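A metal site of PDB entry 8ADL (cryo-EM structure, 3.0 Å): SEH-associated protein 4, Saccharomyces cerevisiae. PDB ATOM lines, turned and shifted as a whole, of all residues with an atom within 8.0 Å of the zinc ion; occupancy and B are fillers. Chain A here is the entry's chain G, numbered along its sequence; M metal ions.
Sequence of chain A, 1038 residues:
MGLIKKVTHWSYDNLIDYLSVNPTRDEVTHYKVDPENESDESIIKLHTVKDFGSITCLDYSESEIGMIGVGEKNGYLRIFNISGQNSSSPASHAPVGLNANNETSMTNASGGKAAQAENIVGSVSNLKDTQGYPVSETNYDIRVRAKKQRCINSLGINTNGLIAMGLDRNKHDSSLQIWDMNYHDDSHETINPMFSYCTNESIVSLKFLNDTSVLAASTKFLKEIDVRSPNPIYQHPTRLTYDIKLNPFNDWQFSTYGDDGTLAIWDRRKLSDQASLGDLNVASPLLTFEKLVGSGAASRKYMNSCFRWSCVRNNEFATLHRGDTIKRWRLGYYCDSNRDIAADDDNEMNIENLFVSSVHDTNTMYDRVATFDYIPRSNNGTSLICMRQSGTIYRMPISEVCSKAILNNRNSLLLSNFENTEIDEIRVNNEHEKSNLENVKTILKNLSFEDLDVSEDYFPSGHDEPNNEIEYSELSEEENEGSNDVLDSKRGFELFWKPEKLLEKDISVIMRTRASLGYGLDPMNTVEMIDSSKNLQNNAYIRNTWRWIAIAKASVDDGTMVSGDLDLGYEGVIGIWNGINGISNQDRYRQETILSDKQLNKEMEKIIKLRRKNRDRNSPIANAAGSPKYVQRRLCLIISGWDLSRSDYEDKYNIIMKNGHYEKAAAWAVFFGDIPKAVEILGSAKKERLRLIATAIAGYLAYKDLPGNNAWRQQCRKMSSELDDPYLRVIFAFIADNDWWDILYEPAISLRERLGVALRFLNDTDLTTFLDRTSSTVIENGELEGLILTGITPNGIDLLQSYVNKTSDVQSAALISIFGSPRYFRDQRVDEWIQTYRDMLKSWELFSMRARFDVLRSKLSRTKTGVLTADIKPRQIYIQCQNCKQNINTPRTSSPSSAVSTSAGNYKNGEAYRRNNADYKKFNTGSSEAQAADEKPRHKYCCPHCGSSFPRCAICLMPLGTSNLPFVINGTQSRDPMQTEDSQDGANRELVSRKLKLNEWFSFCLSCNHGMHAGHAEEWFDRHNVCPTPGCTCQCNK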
ATOM      1  N   GLN A 880      11.184  29.323  30.883  1.00  0.00           N
ATOM      2  CA  GLN A 880      10.605  27.996  30.781  1.00  0.00           C
ATOM      3  C   GLN A 880       9.133  28.103  30.383  1.00  0.00           C
ATOM      4  O   GLN A 880       8.598  29.184  30.150  1.00  0.00           O
ATOM      5  CB  GLN A 880      10.763  27.237  32.097  1.00  0.00           C
ATOM      6  CG  GLN A 880      12.198  26.881  32.445  1.00  0.00           C
ATOM      7  CD  GLN A 880      12.291  25.943  33.630  1.00  0.00           C
ATOM      8  OE1 GLN A 880      11.343  25.796  34.396  1.00  0.00           O
ATOM      9  NE2 GLN A 880      13.445  25.307  33.795  1.00  0.00           N
ATOM     10  N   CYS A 881       8.458  26.945  30.310  1.00  0.00           N
ATOM     11  CA  CYS A 881       7.044  26.897  29.962  1.00  0.00           C
ATOM     12  C   CYS A 881       6.222  26.000  30.877  1.00  0.00           C
ATOM     13  O   CYS A 881       4.994  26.025  30.760  1.00  0.00           O
ATOM     14  CB  CYS A 881       6.853  26.435  28.506  1.00  0.00           C
ATOM     15  SG  CYS A 881       7.079  24.665  28.228  1.00  0.00           S
ATOM     16  N   GLN A 882       6.856  25.181  31.724  1.00  0.00           N
ATOM     17  CA  GLN A 882       6.232  24.345  32.748  1.00  0.00           C
ATOM     18  C   GLN A 882       5.320  23.255  32.162  1.00  0.00           C
ATOM     19  O   GLN A 882       4.612  22.578  32.907  1.00  0.00           O
ATOM     20  CB  GLN A 882       5.458  25.185  33.783  1.00  0.00           C
ATOM     21  CG  GLN A 882       5.470  24.609  35.205  1.00  0.00           C
ATOM     22  CD  GLN A 882       4.614  25.426  36.162  1.00  0.00           C
ATOM     23  OE1 GLN A 882       3.932  26.354  35.755  1.00  0.00           O
ATOM     24  NE2 GLN A 882       4.660  25.056  37.440  1.00  0.00           N
ATOM     25  N   ASN A 883       5.341  23.058  30.846  1.00  0.00           N
ATOM     26  CA  ASN A 883       4.650  21.971  30.186  1.00  0.00           C
ATOM     27  C   ASN A 883       5.589  20.930  29.610  1.00  0.00           C
ATOM     28  O   ASN A 883       5.274  19.739  29.617  1.00  0.00           O
ATOM     29  CB  ASN A 883       3.745  22.512  29.069  1.00  0.00           C
ATOM     30  CG  ASN A 883       2.406  23.009  29.589  1.00  0.00           C
ATOM     31  OD1 ASN A 883       2.000  24.136  29.305  1.00  0.00           O
ATOM     32  ND2 ASN A 883       1.722  22.160  30.349  1.00  0.00           N
ATOM     33  N   CYS A 884       6.758  21.353  29.117  1.00  0.00           N
ATOM     34  CA  CYS A 884       7.858  20.455  28.840  1.00  0.00           C
ATOM     35  C   CYS A 884       9.136  20.838  29.596  1.00  0.00           C
ATOM     36  O   CYS A 884      10.128  20.118  29.487  1.00  0.00           O
ATOM     37  CB  CYS A 884       8.143  20.402  27.339  1.00  0.00           C
ATOM     38  SG  CYS A 884       8.871  21.898  26.642  1.00  0.00           S
ATOM     39  N   LYS A 885       9.107  21.945  30.353  1.00  0.00           N
ATOM     40  CA  LYS A 885      10.212  22.415  31.183  1.00  0.00           C
ATOM     41  C   LYS A 885      11.494  22.616  30.375  1.00  0.00           C
ATOM     42  O   LYS A 885      12.581  22.171  30.748  1.00  0.00           O
ATOM     43  CB  LYS A 885      10.463  21.470  32.360  1.00  0.00           C
ATOM     44  CG  LYS A 885       9.343  21.446  33.387  1.00  0.00           C
ATOM     45  CD  LYS A 885       9.598  20.404  34.456  1.00  0.00           C
ATOM     46  CE  LYS A 885       8.442  20.346  35.455  1.00  0.00           C
ATOM     47  NZ  LYS A 885       8.657  19.300  36.491  1.00  0.00           N
ATOM     48  N   GLN A 886      11.363  23.315  29.246  1.00  0.00           N
ATOM     49  CA  GLN A 886      12.482  23.622  28.369  1.00  0.00           C
ATOM     50  C   GLN A 886      12.460  25.099  28.013  1.00  0.00           C
ATOM     51  O   GLN A 886      11.516  25.824  28.333  1.00  0.00           O
ATOM     52  CB  GLN A 886      12.440  22.774  27.082  1.00  0.00           C
ATOM     53  CG  GLN A 886      12.588  21.280  27.305  1.00  0.00           C
ATOM     54  CD  GLN A 886      14.031  20.860  27.500  1.00  0.00           C
ATOM     55  OE1 GLN A 886      14.913  21.253  26.735  1.00  0.00           O
ATOM     56  NE2 GLN A 886      14.277  20.043  28.515  1.00  0.00           N
ATOM     57  N   ASN A 887      13.529  25.535  27.351  1.00  0.00           N
ATOM     58  CA  ASN A 887      13.600  26.902  26.859  1.00  0.00           C
ATOM     59  C   ASN A 887      12.632  27.094  25.713  1.00  0.00           C
ATOM     60  O   ASN A 887      12.446  26.203  24.876  1.00  0.00           O
ATOM     61  CB  ASN A 887      15.028  27.229  26.425  1.00  0.00           C
ATOM     62  CG  ASN A 887      15.311  28.722  26.437  1.00  0.00           C
ATOM     63  OD1 ASN A 887      14.459  29.526  26.826  1.00  0.00           O
ATOM     64  ND2 ASN A 887      16.512  29.107  26.016  1.00  0.00           N
ATOM     65  N   ILE A 888      11.989  28.269  25.656  1.00  0.00           N
ATOM     66  CA  ILE A 888      11.024  28.532  24.600  1.00  0.00           C
ATOM     67  C   ILE A 888      11.668  29.162  23.370  1.00  0.00           C
ATOM     68  O   ILE A 888      10.973  29.386  22.363  1.00  0.00           O
ATOM     69  CB  ILE A 888       9.884  29.458  25.088  1.00  0.00           C
ATOM     70  CG1 ILE A 888      10.378  30.897  25.204  1.00  0.00           C
ATOM     71  CG2 ILE A 888       9.352  28.965  26.423  1.00  0.00           C
ATOM     72  CD1 ILE A 888       9.259  31.906  25.243  1.00  0.00           C
ATOM     73  N   CYS A 942       3.584  29.644  20.095  1.00  0.00           N
ATOM     74  CA  CYS A 942       3.473  28.357  20.777  1.00  0.00           C
ATOM     75  C   CYS A 942       4.864  27.908  21.194  1.00  0.00           C
ATOM     76  O   CYS A 942       5.880  28.400  20.675  1.00  0.00           O
ATOM     77  CB  CYS A 942       2.818  27.295  19.891  1.00  0.00           C
ATOM     78  SG  CYS A 942       1.022  27.347  19.865  1.00  0.00           S
ATOM     79  N   CYS A 943       4.914  26.990  22.149  1.00  0.00           N
ATOM     80  CA  CYS A 943       6.203  26.460  22.585  1.00  0.00           C
ATOM     81  C   CYS A 943       6.791  25.568  21.493  1.00  0.00           C
ATOM     82  O   CYS A 943       6.080  24.715  20.953  1.00  0.00           O
ATOM     83  CB  CYS A 943       6.042  25.661  23.884  1.00  0.00           C
ATOM     84  SG  CYS A 943       7.553  24.833  24.436  1.00  0.00           S
ATOM     85  N   PRO A 944       8.063  25.741  21.141  1.00  0.00           N
ATOM     86  CA  PRO A 944       8.658  24.956  20.059  1.00  0.00           C
ATOM     87  C   PRO A 944       9.044  23.526  20.441  1.00  0.00           C
ATOM     88  O   PRO A 944       9.618  22.824  19.606  1.00  0.00           O
ATOM     89  CB  PRO A 944       9.918  25.769  19.681  1.00  0.00           C
ATOM     90  CG  PRO A 944       9.754  27.089  20.372  1.00  0.00           C
ATOM     91  CD  PRO A 944       8.969  26.799  21.605  1.00  0.00           C
ATOM     92  N   HIS A 945       8.748  23.089  21.663  1.00  0.00           N
ATOM     93  CA  HIS A 945       9.053  21.720  22.057  1.00  0.00           C
ATOM     94  C   HIS A 945       7.843  20.911  22.531  1.00  0.00           C
ATOM     95  O   HIS A 945       7.915  19.680  22.519  1.00  0.00           O
ATOM     96  CB  HIS A 945      10.101  21.713  23.190  1.00  0.00           C
ATOM     97  CG  HIS A 945      11.421  22.286  22.788  1.00  0.00           C
ATOM     98  ND1 HIS A 945      11.860  22.305  21.479  1.00  0.00           N
ATOM     99  CD2 HIS A 945      12.400  22.876  23.519  1.00  0.00           C
ATOM    100  CE1 HIS A 945      13.052  22.868  21.430  1.00  0.00           C
ATOM    101  NE2 HIS A 945      13.405  23.226  22.655  1.00  0.00           N
ATOM    102  N   CYS A 946       6.753  21.566  22.937  1.00  0.00           N
ATOM    103  CA  CYS A 946       5.552  20.832  23.326  1.00  0.00           C
ATOM    104  C   CYS A 946       4.269  21.431  22.766  1.00  0.00           C
ATOM    105  O   CYS A 946       3.206  20.850  22.982  1.00  0.00           O
ATOM    106  CB  CYS A 946       5.452  20.750  24.860  1.00  0.00           C
ATOM    107  SG  CYS A 946       5.175  22.329  25.699  1.00  0.00           S
ATOM    108  N   GLY A 947       4.335  22.568  22.074  1.00  0.00           N
ATOM    109  CA  GLY A 947       3.176  23.124  21.415  1.00  0.00           C
ATOM    110  C   GLY A 947       2.159  23.791  22.332  1.00  0.00           C
ATOM    111  O   GLY A 947       1.089  24.165  21.863  1.00  0.00           O
ATOM    112  N   SER A 948       2.470  23.922  23.613  1.00  0.00           N
ATOM    113  CA  SER A 948       1.529  24.531  24.547  1.00  0.00           C
ATOM    114  C   SER A 948       1.416  26.032  24.289  1.00  0.00           C
ATOM    115  O   SER A 948       2.336  26.665  23.752  1.00  0.00           O
ATOM    116  CB  SER A 948       1.969  24.286  25.993  1.00  0.00           C
ATOM    117  OG  SER A 948       1.022  24.797  26.906  1.00  0.00           O
ATOM    118  N   SER A 949       0.278  26.598  24.658  1.00  0.00           N
ATOM    119  CA  SER A 949      -0.006  27.986  24.333  1.00  0.00           C
ATOM    120  C   SER A 949       0.764  28.928  25.238  1.00  0.00           C
ATOM    121  O   SER A 949       0.851  28.719  26.446  1.00  0.00           O
ATOM    122  CB  SER A 949      -1.511  28.262  24.459  1.00  0.00           C
ATOM    123  OG  SER A 949      -2.246  27.552  23.475  1.00  0.00           O
ATOM    124  N   PHE A 950       1.335  29.970  24.629  1.00  0.00           N
ATOM    125  CA  PHE A 950       2.038  30.981  25.384  1.00  0.00           C
ATOM    126  C   PHE A 950       1.036  31.888  26.102  1.00  0.00           C
ATOM    127  O   PHE A 950      -0.094  32.070  25.634  1.00  0.00           O
ATOM    128  CB  PHE A 950       2.928  31.818  24.474  1.00  0.00           C
ATOM    129  CG  PHE A 950       4.231  31.164  24.135  1.00  0.00           C
ATOM    130  CD1 PHE A 950       4.716  30.098  24.880  1.00  0.00           C
ATOM    131  CD2 PHE A 950       4.984  31.613  23.054  1.00  0.00           C
ATOM    132  CE1 PHE A 950       5.915  29.497  24.570  1.00  0.00           C
ATOM    133  CE2 PHE A 950       6.191  31.015  22.738  1.00  0.00           C
ATOM    134  CZ  PHE A 950       6.649  29.954  23.502  1.00  0.00           C
HETATM  135 ZN    ZN M   1       7.162  23.427  26.260  1.00  0.00          ZN
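The backbone NH (N) of Asn 883 sits close to the side-chain sulfur (SG) of Cys 881 (3.5 Å). The backbone NH (N) of His 945 sits close to the side-chain sulfur (SG) of Cys 943 (3.5 Å). O of Ser 948 is in hydrogen-bond range of N of Cys 943 (3.1 Å). SG of Cys 946 sits close to N of Ser 948, 3.8 Å away.
The zinc ion is bound by the side-chain sulfur of Cys 884 (2.3 Å), the side-chain sulfur of Cys 881 (2.3 Å), the side-chain sulfur of Cys 943 (2.3 Å) and the side-chain sulfur of Cys 946 (2.3 Å).
Within 4 Å of the zinc ion: Cys 881, Cys 884, Cys 943 and Cys 946.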
